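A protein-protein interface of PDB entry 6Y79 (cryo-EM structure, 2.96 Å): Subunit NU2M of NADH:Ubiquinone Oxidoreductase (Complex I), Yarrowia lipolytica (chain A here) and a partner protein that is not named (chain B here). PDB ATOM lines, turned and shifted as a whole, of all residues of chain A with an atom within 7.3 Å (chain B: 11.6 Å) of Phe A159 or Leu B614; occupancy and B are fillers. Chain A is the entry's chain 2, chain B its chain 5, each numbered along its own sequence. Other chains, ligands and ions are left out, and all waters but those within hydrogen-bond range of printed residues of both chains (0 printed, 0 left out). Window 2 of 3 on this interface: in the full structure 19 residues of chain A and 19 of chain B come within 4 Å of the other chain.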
ATOM      1  N   TYR A 138       0.214  -5.959 -17.974  1.00  0.00           N
ATOM      2  CA  TYR A 138       0.783  -4.650 -17.615  1.00  0.00           C
ATOM      3  C   TYR A 138       0.871  -4.476 -16.103  1.00  0.00           C
ATOM      4  O   TYR A 138       1.918  -4.109 -15.558  1.00  0.00           O
ATOM      5  CB  TYR A 138      -0.062  -3.490 -18.156  1.00  0.00           C
ATOM      6  CG  TYR A 138      -0.340  -3.382 -19.635  1.00  0.00           C
ATOM      7  CD1 TYR A 138       0.425  -4.029 -20.554  1.00  0.00           C
ATOM      8  CD2 TYR A 138      -1.372  -2.586 -20.099  1.00  0.00           C
ATOM      9  CE1 TYR A 138       0.169  -3.943 -21.899  1.00  0.00           C
ATOM     10  CE2 TYR A 138      -1.643  -2.482 -21.438  1.00  0.00           C
ATOM     11  CZ  TYR A 138      -0.860  -3.158 -22.335  1.00  0.00           C
ATOM     12  OH  TYR A 138      -1.118  -3.052 -23.675  1.00  0.00           O
ATOM     13  N   ALA A 153      10.285  -2.438 -17.629  1.00  0.00           N
ATOM     14  CA  ALA A 153       9.689  -3.526 -18.391  1.00  0.00           C
ATOM     15  C   ALA A 153       8.193  -3.335 -18.563  1.00  0.00           C
ATOM     16  O   ALA A 153       7.652  -3.631 -19.631  1.00  0.00           O
ATOM     17  CB  ALA A 153       9.981  -4.855 -17.705  1.00  0.00           C
ATOM     18  N   SER A 154       7.508  -2.833 -17.534  1.00  0.00           N
ATOM     19  CA  SER A 154       6.075  -2.582 -17.649  1.00  0.00           C
ATOM     20  C   SER A 154       5.777  -1.455 -18.624  1.00  0.00           C
ATOM     21  O   SER A 154       4.787  -1.518 -19.363  1.00  0.00           O
ATOM     22  CB  SER A 154       5.492  -2.259 -16.286  1.00  0.00           C
ATOM     23  OG  SER A 154       5.984  -1.021 -15.824  1.00  0.00           O
ATOM     24  N   MET A 155       6.635  -0.434 -18.666  1.00  0.00           N
ATOM     25  CA  MET A 155       6.442   0.636 -19.645  1.00  0.00           C
ATOM     26  C   MET A 155       6.651   0.136 -21.071  1.00  0.00           C
ATOM     27  O   MET A 155       5.841   0.421 -21.972  1.00  0.00           O
ATOM     28  CB  MET A 155       7.382   1.794 -19.339  1.00  0.00           C
ATOM     29  CG  MET A 155       7.023   2.532 -18.076  1.00  0.00           C
ATOM     30  SD  MET A 155       5.341   3.142 -18.117  1.00  0.00           S
ATOM     31  CE  MET A 155       5.448   4.275 -19.485  1.00  0.00           C
ATOM     32  N   LEU A 156       7.727  -0.631 -21.283  1.00  0.00           N
ATOM     33  CA  LEU A 156       8.012  -1.203 -22.596  1.00  0.00           C
ATOM     34  C   LEU A 156       6.901  -2.136 -23.051  1.00  0.00           C
ATOM     35  O   LEU A 156       6.484  -2.101 -24.217  1.00  0.00           O
ATOM     36  CB  LEU A 156       9.343  -1.947 -22.540  1.00  0.00           C
ATOM     37  CG  LEU A 156      10.080  -2.354 -23.808  1.00  0.00           C
ATOM     38  CD1 LEU A 156      11.527  -2.305 -23.514  1.00  0.00           C
ATOM     39  CD2 LEU A 156       9.757  -3.738 -24.164  1.00  0.00           C
ATOM     40  N   TYR A 157       6.398  -2.960 -22.135  1.00  0.00           N
ATOM     41  CA  TYR A 157       5.340  -3.891 -22.475  1.00  0.00           C
ATOM     42  C   TYR A 157       4.037  -3.172 -22.761  1.00  0.00           C
ATOM     43  O   TYR A 157       3.286  -3.617 -23.631  1.00  0.00           O
ATOM     44  CB  TYR A 157       5.159  -4.915 -21.358  1.00  0.00           C
ATOM     45  CG  TYR A 157       4.209  -6.009 -21.740  1.00  0.00           C
ATOM     46  CD1 TYR A 157       4.555  -7.011 -22.627  1.00  0.00           C
ATOM     47  CD2 TYR A 157       2.959  -6.018 -21.233  1.00  0.00           C
ATOM     48  CE1 TYR A 157       3.656  -7.991 -22.976  1.00  0.00           C
ATOM     49  CE2 TYR A 157       2.039  -6.951 -21.595  1.00  0.00           C
ATOM     50  CZ  TYR A 157       2.396  -7.958 -22.444  1.00  0.00           C
ATOM     51  OH  TYR A 157       1.464  -8.913 -22.767  1.00  0.00           O
ATOM     52  N   PHE A 158       3.781  -2.045 -22.086  1.00  0.00           N
ATOM     53  CA  PHE A 158       2.609  -1.230 -22.389  1.00  0.00           C
ATOM     54  C   PHE A 158       2.628  -0.726 -23.822  1.00  0.00           C
ATOM     55  O   PHE A 158       1.642  -0.870 -24.551  1.00  0.00           O
ATOM     56  CB  PHE A 158       2.526  -0.045 -21.435  1.00  0.00           C
ATOM     57  CG  PHE A 158       1.374   0.863 -21.722  1.00  0.00           C
ATOM     58  CD1 PHE A 158       0.106   0.494 -21.353  1.00  0.00           C
ATOM     59  CD2 PHE A 158       1.552   2.079 -22.369  1.00  0.00           C
ATOM     60  CE1 PHE A 158      -0.957   1.293 -21.622  1.00  0.00           C
ATOM     61  CE2 PHE A 158       0.476   2.884 -22.639  1.00  0.00           C
ATOM     62  CZ  PHE A 158      -0.779   2.491 -22.261  1.00  0.00           C
ATOM     63  N   PHE A 159       3.746  -0.135 -24.248  1.00  0.00           N
ATOM     64  CA  PHE A 159       3.767   0.453 -25.590  1.00  0.00           C
ATOM     65  C   PHE A 159       3.778  -0.612 -26.683  1.00  0.00           C
ATOM     66  O   PHE A 159       3.062  -0.487 -27.696  1.00  0.00           O
ATOM     67  CB  PHE A 159       4.957   1.383 -25.736  1.00  0.00           C
ATOM     68  CG  PHE A 159       4.813   2.649 -24.967  1.00  0.00           C
ATOM     69  CD1 PHE A 159       3.882   3.597 -25.341  1.00  0.00           C
ATOM     70  CD2 PHE A 159       5.601   2.890 -23.864  1.00  0.00           C
ATOM     71  CE1 PHE A 159       3.744   4.749 -24.627  1.00  0.00           C
ATOM     72  CE2 PHE A 159       5.463   4.041 -23.148  1.00  0.00           C
ATOM     73  CZ  PHE A 159       4.539   4.969 -23.533  1.00  0.00           C
ATOM     74  N   MET A 160       4.545  -1.685 -26.486  1.00  0.00           N
ATOM     75  CA  MET A 160       4.581  -2.728 -27.499  1.00  0.00           C
ATOM     76  C   MET A 160       3.323  -3.585 -27.514  1.00  0.00           C
ATOM     77  O   MET A 160       3.047  -4.217 -28.533  1.00  0.00           O
ATOM     78  CB  MET A 160       5.800  -3.608 -27.298  1.00  0.00           C
ATOM     79  CG  MET A 160       7.114  -2.881 -27.325  1.00  0.00           C
ATOM     80  SD  MET A 160       7.609  -2.364 -28.960  1.00  0.00           S
ATOM     81  CE  MET A 160       7.377  -0.597 -28.834  1.00  0.00           C
ATOM     82  N   GLY A 161       2.548  -3.625 -26.429  1.00  0.00           N
ATOM     83  CA  GLY A 161       1.247  -4.256 -26.498  1.00  0.00           C
ATOM     84  C   GLY A 161       0.186  -3.348 -27.073  1.00  0.00           C
ATOM     85  O   GLY A 161      -0.755  -3.827 -27.714  1.00  0.00           O
ATOM     86  N   GLY A 162       0.337  -2.034 -26.884  1.00  0.00           N
ATOM     87  CA  GLY A 162      -0.609  -1.097 -27.461  1.00  0.00           C
ATOM     88  C   GLY A 162      -0.582  -1.083 -28.974  1.00  0.00           C
ATOM     89  O   GLY A 162      -1.642  -1.076 -29.611  1.00  0.00           O
ATOM     90  N   ILE A 163       0.622  -1.103 -29.568  1.00  0.00           N
ATOM     91  CA  ILE A 163       0.734  -1.153 -31.033  1.00  0.00           C
ATOM     92  C   ILE A 163       0.083  -2.412 -31.588  1.00  0.00           C
ATOM     93  O   ILE A 163      -0.702  -2.367 -32.542  1.00  0.00           O
ATOM     94  CB  ILE A 163       2.200  -1.098 -31.484  1.00  0.00           C
ATOM     95  CG1 ILE A 163       2.929   0.114 -30.968  1.00  0.00           C
ATOM     96  CG2 ILE A 163       2.289  -1.111 -33.000  1.00  0.00           C
ATOM     97  CD1 ILE A 163       4.405  -0.075 -31.180  1.00  0.00           C
ATOM     98  N   LEU A 164       0.401  -3.553 -31.000  1.00  0.00           N
ATOM     99  CA  LEU A 164      -0.058  -4.818 -31.537  1.00  0.00           C
ATOM    100  C   LEU A 164      -1.489  -5.129 -31.157  1.00  0.00           C
ATOM    101  O   LEU A 164      -2.024  -6.136 -31.624  1.00  0.00           O
ATOM    102  CB  LEU A 164       0.874  -5.930 -31.074  1.00  0.00           C
ATOM    103  CG  LEU A 164       2.257  -5.609 -31.614  1.00  0.00           C
ATOM    104  CD1 LEU A 164       3.295  -6.456 -30.947  1.00  0.00           C
ATOM    105  CD2 LEU A 164       2.284  -5.782 -33.121  1.00  0.00           C
ATOM    106  N   SER A 165      -2.098  -4.314 -30.299  1.00  0.00           N
ATOM    107  CA  SER A 165      -3.541  -4.351 -30.117  1.00  0.00           C
ATOM    108  C   SER A 165      -4.272  -3.477 -31.117  1.00  0.00           C
ATOM    109  O   SER A 165      -5.353  -3.845 -31.593  1.00  0.00           O
ATOM    110  CB  SER A 165      -3.875  -3.919 -28.708  1.00  0.00           C
ATOM    111  OG  SER A 165      -3.538  -4.969 -27.817  1.00  0.00           O
ATOM    112  N   TRP A 220      12.060  -7.454 -27.480  1.00  0.00           N
ATOM    113  CA  TRP A 220      11.383  -6.707 -26.435  1.00  0.00           C
ATOM    114  C   TRP A 220      10.789  -7.645 -25.390  1.00  0.00           C
ATOM    115  O   TRP A 220      10.882  -7.378 -24.189  1.00  0.00           O
ATOM    116  CB  TRP A 220      10.323  -5.804 -27.063  1.00  0.00           C
ATOM    117  CG  TRP A 220       9.260  -6.508 -27.808  1.00  0.00           C
ATOM    118  CD1 TRP A 220       9.332  -6.979 -29.071  1.00  0.00           C
ATOM    119  CD2 TRP A 220       7.948  -6.815 -27.338  1.00  0.00           C
ATOM    120  NE1 TRP A 220       8.152  -7.574 -29.423  1.00  0.00           N
ATOM    121  CE2 TRP A 220       7.283  -7.483 -28.371  1.00  0.00           C
ATOM    122  CE3 TRP A 220       7.273  -6.595 -26.137  1.00  0.00           C
ATOM    123  CZ2 TRP A 220       5.980  -7.931 -28.243  1.00  0.00           C
ATOM    124  CZ3 TRP A 220       5.981  -7.034 -26.015  1.00  0.00           C
ATOM    125  CH2 TRP A 220       5.346  -7.694 -27.058  1.00  0.00           C
ATOM    126  N   SER B 607      20.291  -5.599 -31.733  1.00  0.00           N
ATOM    127  CA  SER B 607      19.696  -4.478 -31.004  1.00  0.00           C
ATOM    128  C   SER B 607      20.637  -3.893 -29.955  1.00  0.00           C
ATOM    129  O   SER B 607      20.230  -3.587 -28.832  1.00  0.00           O
ATOM    130  CB  SER B 607      18.393  -4.896 -30.346  1.00  0.00           C
ATOM    131  OG  SER B 607      18.646  -5.755 -29.252  1.00  0.00           O
ATOM    132  N   SER B 608      21.906  -3.735 -30.309  1.00  0.00           N
ATOM    133  CA  SER B 608      22.901  -3.207 -29.389  1.00  0.00           C
ATOM    134  C   SER B 608      22.945  -1.685 -29.397  1.00  0.00           C
ATOM    135  O   SER B 608      23.371  -1.077 -28.406  1.00  0.00           O
ATOM    136  CB  SER B 608      24.279  -3.759 -29.751  1.00  0.00           C
ATOM    137  OG  SER B 608      24.623  -3.397 -31.081  1.00  0.00           O
ATOM    138  N   ASN B 609      22.469  -1.079 -30.494  1.00  0.00           N
ATOM    139  CA  ASN B 609      22.829   0.279 -30.892  1.00  0.00           C
ATOM    140  C   ASN B 609      22.358   1.333 -29.904  1.00  0.00           C
ATOM    141  O   ASN B 609      23.169   1.993 -29.244  1.00  0.00           O
ATOM    142  CB  ASN B 609      22.218   0.589 -32.260  1.00  0.00           C
ATOM    143  CG  ASN B 609      23.062   0.095 -33.407  1.00  0.00           C
ATOM    144  OD1 ASN B 609      22.641  -0.774 -34.169  1.00  0.00           O
ATOM    145  ND2 ASN B 609      24.253   0.661 -33.553  1.00  0.00           N
ATOM    146  N   THR B 610      21.049   1.484 -29.778  1.00  0.00           N
ATOM    147  CA  THR B 610      20.490   2.727 -29.285  1.00  0.00           C
ATOM    148  C   THR B 610      20.439   2.718 -27.760  1.00  0.00           C
ATOM    149  O   THR B 610      20.240   1.677 -27.125  1.00  0.00           O
ATOM    150  CB  THR B 610      19.099   2.930 -29.913  1.00  0.00           C
ATOM    151  OG1 THR B 610      19.204   2.741 -31.329  1.00  0.00           O
ATOM    152  CG2 THR B 610      18.539   4.332 -29.669  1.00  0.00           C
ATOM    153  N   ARG B 611      20.657   3.906 -27.179  1.00  0.00           N
ATOM    154  CA  ARG B 611      20.397   4.151 -25.761  1.00  0.00           C
ATOM    155  C   ARG B 611      18.951   3.821 -25.383  1.00  0.00           C
ATOM    156  O   ARG B 611      18.675   3.409 -24.250  1.00  0.00           O
ATOM    157  CB  ARG B 611      20.707   5.619 -25.449  1.00  0.00           C
ATOM    158  CG  ARG B 611      20.715   5.989 -23.984  1.00  0.00           C
ATOM    159  CD  ARG B 611      21.808   5.264 -23.251  1.00  0.00           C
ATOM    160  NE  ARG B 611      23.123   5.679 -23.718  1.00  0.00           N
ATOM    161  CZ  ARG B 611      24.258   5.095 -23.356  1.00  0.00           C
ATOM    162  NH1 ARG B 611      25.415   5.537 -23.830  1.00  0.00           N
ATOM    163  NH2 ARG B 611      24.237   4.072 -22.515  1.00  0.00           N
ATOM    164  N   SER B 612      18.018   3.984 -26.323  1.00  0.00           N
ATOM    165  CA  SER B 612      16.595   3.817 -26.068  1.00  0.00           C
ATOM    166  C   SER B 612      16.156   2.380 -26.302  1.00  0.00           C
ATOM    167  O   SER B 612      16.517   1.772 -27.314  1.00  0.00           O
ATOM    168  CB  SER B 612      15.771   4.743 -26.949  1.00  0.00           C
ATOM    169  OG  SER B 612      14.427   4.287 -27.028  1.00  0.00           O
ATOM    170  N   SER B 613      15.373   1.843 -25.355  1.00  0.00           N
ATOM    171  CA  SER B 613      14.698   0.577 -25.591  1.00  0.00           C
ATOM    172  C   SER B 613      13.514   0.787 -26.526  1.00  0.00           C
ATOM    173  O   SER B 613      13.302   0.018 -27.473  1.00  0.00           O
ATOM    174  CB  SER B 613      14.248   0.001 -24.265  1.00  0.00           C
ATOM    175  OG  SER B 613      15.306  -0.062 -23.298  1.00  0.00           O
ATOM    176  N   LEU B 614      12.765   1.863 -26.297  1.00  0.00           N
ATOM    177  CA  LEU B 614      11.436   2.022 -26.874  1.00  0.00           C
ATOM    178  C   LEU B 614      11.488   2.444 -28.335  1.00  0.00           C
ATOM    179  O   LEU B 614      10.730   1.926 -29.161  1.00  0.00           O
ATOM    180  CB  LEU B 614      10.652   3.034 -26.047  1.00  0.00           C
ATOM    181  CG  LEU B 614       9.220   3.244 -26.469  1.00  0.00           C
ATOM    182  CD1 LEU B 614       8.497   1.940 -26.335  1.00  0.00           C
ATOM    183  CD2 LEU B 614       8.611   4.283 -25.582  1.00  0.00           C
ATOM    184  N   SER B 615      12.351   3.411 -28.665  1.00  0.00           N
ATOM    185  CA  SER B 615      12.498   3.858 -30.046  1.00  0.00           C
ATOM    186  C   SER B 615      13.062   2.750 -30.915  1.00  0.00           C
ATOM    187  O   SER B 615      12.622   2.565 -32.056  1.00  0.00           O
ATOM    188  CB  SER B 615      13.402   5.083 -30.107  1.00  0.00           C
ATOM    189  OG  SER B 615      14.766   4.703 -30.204  1.00  0.00           O
ATOM    190  N   MET B 616      14.019   1.995 -30.364  1.00  0.00           N
ATOM    191  CA  MET B 616      14.586   0.817 -31.006  1.00  0.00           C
ATOM    192  C   MET B 616      13.513  -0.192 -31.379  1.00  0.00           C
ATOM    193  O   MET B 616      13.378  -0.566 -32.553  1.00  0.00           O
ATOM    194  CB  MET B 616      15.609   0.198 -30.060  1.00  0.00           C
ATOM    195  CG  MET B 616      16.110  -1.168 -30.431  1.00  0.00           C
ATOM    196  SD  MET B 616      16.886  -1.910 -28.983  1.00  0.00           S
ATOM    197  CE  MET B 616      18.324  -0.858 -28.803  1.00  0.00           C
ATOM    198  N   ASN B 617      12.701  -0.605 -30.400  1.00  0.00           N
ATOM    199  CA  ASN B 617      11.716  -1.642 -30.689  1.00  0.00           C
ATOM    200  C   ASN B 617      10.541  -1.128 -31.516  1.00  0.00           C
ATOM    201  O   ASN B 617      10.011  -1.870 -32.348  1.00  0.00           O
ATOM    202  CB  ASN B 617      11.239  -2.264 -29.388  1.00  0.00           C
ATOM    203  CG  ASN B 617      12.336  -3.008 -28.683  1.00  0.00           C
ATOM    204  OD1 ASN B 617      12.986  -3.869 -29.268  1.00  0.00           O
ATOM    205  ND2 ASN B 617      12.572  -2.665 -27.431  1.00  0.00           N
ATOM    206  N   SER B 618      10.131   0.131 -31.346  1.00  0.00           N
ATOM    207  CA  SER B 618       9.023   0.635 -32.149  1.00  0.00           C
ATOM    208  C   SER B 618       9.432   0.977 -33.574  1.00  0.00           C
ATOM    209  O   SER B 618       8.573   0.974 -34.458  1.00  0.00           O
ATOM    210  CB  SER B 618       8.382   1.848 -31.470  1.00  0.00           C
ATOM    211  OG  SER B 618       9.292   2.917 -31.322  1.00  0.00           O
ATOM    212  N   MET B 619      10.710   1.253 -33.833  1.00  0.00           N
ATOM    213  CA  MET B 619      11.162   1.311 -35.215  1.00  0.00           C
ATOM    214  C   MET B 619      11.310  -0.076 -35.807  1.00  0.00           C
ATOM    215  O   MET B 619      11.062  -0.271 -37.007  1.00  0.00           O
ATOM    216  CB  MET B 619      12.488   2.066 -35.312  1.00  0.00           C
ATOM    217  CG  MET B 619      12.371   3.578 -35.200  1.00  0.00           C
ATOM    218  SD  MET B 619      13.893   4.482 -35.519  1.00  0.00           S
ATOM    219  CE  MET B 619      14.836   4.126 -34.044  1.00  0.00           C
ATOM    220  N   LEU B 620      11.675  -1.043 -34.964  1.00  0.00           N
ATOM    221  CA  LEU B 620      11.765  -2.432 -35.385  1.00  0.00           C
ATOM    222  C   LEU B 620      10.412  -3.006 -35.784  1.00  0.00           C
ATOM    223  O   LEU B 620      10.348  -3.841 -36.684  1.00  0.00           O
ATOM    224  CB  LEU B 620      12.381  -3.248 -34.254  1.00  0.00           C
ATOM    225  CG  LEU B 620      12.823  -4.676 -34.514  1.00  0.00           C
ATOM    226  CD1 LEU B 620      13.736  -4.685 -35.699  1.00  0.00           C
ATOM    227  CD2 LEU B 620      13.540  -5.194 -33.295  1.00  0.00           C
ATOM    228  N   ILE B 621       9.327  -2.582 -35.132  1.00  0.00           N
ATOM    229  CA  ILE B 621       7.993  -3.022 -35.552  1.00  0.00           C
ATOM    230  C   ILE B 621       7.632  -2.438 -36.913  1.00  0.00           C
ATOM    231  O   ILE B 621       7.025  -3.122 -37.748  1.00  0.00           O
ATOM    232  CB  ILE B 621       6.937  -2.661 -34.486  1.00  0.00           C
ATOM    233  CG1 ILE B 621       7.245  -3.368 -33.172  1.00  0.00           C
ATOM    234  CG2 ILE B 621       5.523  -3.032 -34.941  1.00  0.00           C
ATOM    235  CD1 ILE B 621       6.154  -3.258 -32.143  1.00  0.00           C
ATOM    236  N   LEU B 622       8.025  -1.187 -37.170  1.00  0.00           N
ATOM    237  CA  LEU B 622       7.742  -0.546 -38.450  1.00  0.00           C
ATOM    238  C   LEU B 622       8.462  -1.248 -39.591  1.00  0.00           C
ATOM    239  O   LEU B 622       7.871  -1.468 -40.660  1.00  0.00           O
ATOM    240  CB  LEU B 622       8.154   0.925 -38.406  1.00  0.00           C
ATOM    241  CG  LEU B 622       8.127   1.626 -39.764  1.00  0.00           C
ATOM    242  CD1 LEU B 622       6.707   1.750 -40.253  1.00  0.00           C
ATOM    243  CD2 LEU B 622       8.801   2.959 -39.731  1.00  0.00           C
ATOM    244  N   ILE B 623       9.735  -1.614 -39.365  1.00  0.00           N
ATOM    245  CA  ILE B 623      10.562  -2.213 -40.414  1.00  0.00           C
ATOM    246  C   ILE B 623       9.940  -3.499 -40.937  1.00  0.00           C
ATOM    247  O   ILE B 623       9.863  -3.708 -42.147  1.00  0.00           O
ATOM    248  CB  ILE B 623      11.996  -2.458 -39.911  1.00  0.00           C
ATOM    249  CG1 ILE B 623      12.729  -1.148 -39.693  1.00  0.00           C
ATOM    250  CG2 ILE B 623      12.789  -3.299 -40.905  1.00  0.00           C
ATOM    251  CD1 ILE B 623      14.116  -1.358 -39.196  1.00  0.00           C
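Hydrophobic or aromatic side chains of chain B that line the printed part of chain A: Leu B614 and Ile B621.
Of the 15 printed residues of chain A, 5 touch a printed residue of chain B.
Hydrophobic or aromatic side chains of chain A that line the printed part of chain B: Leu A156, Phe A159, Met A160, Ile A163 and Trp A220.
Along chain A the printed residues that touch a printed residue of chain B span positions 156 to 220.
Among the printed residues, 8 pairs touch across the chains.
Among the printed residues, pairs that only touch across the chains: Leu A156 with Ser B613 (3.6 Å), Phe A159 with Leu B614 (3.6 Å), Met A160 with Leu B614 (3.7 Å), Met A160 with Asn B617 (3.7 Å), Met A160 with Ser B618 (3.7 Å), Met A160 with Ile B621 (3.6 Å), Ile A163 with Ile B621 (3.8 Å) and Trp A220 with Asn B617 (3.8 Å).
The side-chain hydroxyl of Ser B612 is in hydrogen-bond range of the backbone NH of Leu B614 (3.0 Å).
O of Ser B613 is in hydrogen-bond range of ND2 of Asn B617 (2.8 Å).
O of Leu B614 sits at hydrogen-bond distance from OG of Ser B618.
The backbone carbonyl oxygen (O) of Ser B615 is in hydrogen-bond range of the side-chain hydroxyl (OG) of Ser B618 (3.4 Å).
No residue of chain B comes within 4 Å of Met A155.
Leu A156 touches just one residue of chain B: Ser B613 (3.6 Å).
Of the printed residues of chain B, Phe A159 touches Leu B614 (3.6 Å).
Met A160 touches four residues of chain B.
No residue of chain B comes within 4 Å of Gly A161.
No residue of chain B comes within 4 Å of Gly A162.
Of the printed residues of chain B, Trp A220 touches Asn B617.
Printed residues of chain A within 4 Å of Ser B613: Leu A156 (3.6 Å).
Of chain A, only Phe A159 (3.6 Å) and Met A160 (3.7 Å) come within 4 Å of Leu B614.
Of the printed residues of chain A, Asn B617 touches Met A160 and Trp A220.
Of the printed residues of chain A, Ile B621 touches Met A160 (3.6 Å) and Ile A163 (3.8 Å).
The nearest residue of chain B that does not touch Phe A159 is Ile B621 (6.1 Å).
The nearest printed residue of chain A that does not touch Ile B621 is Leu A164 (4.5 Å).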
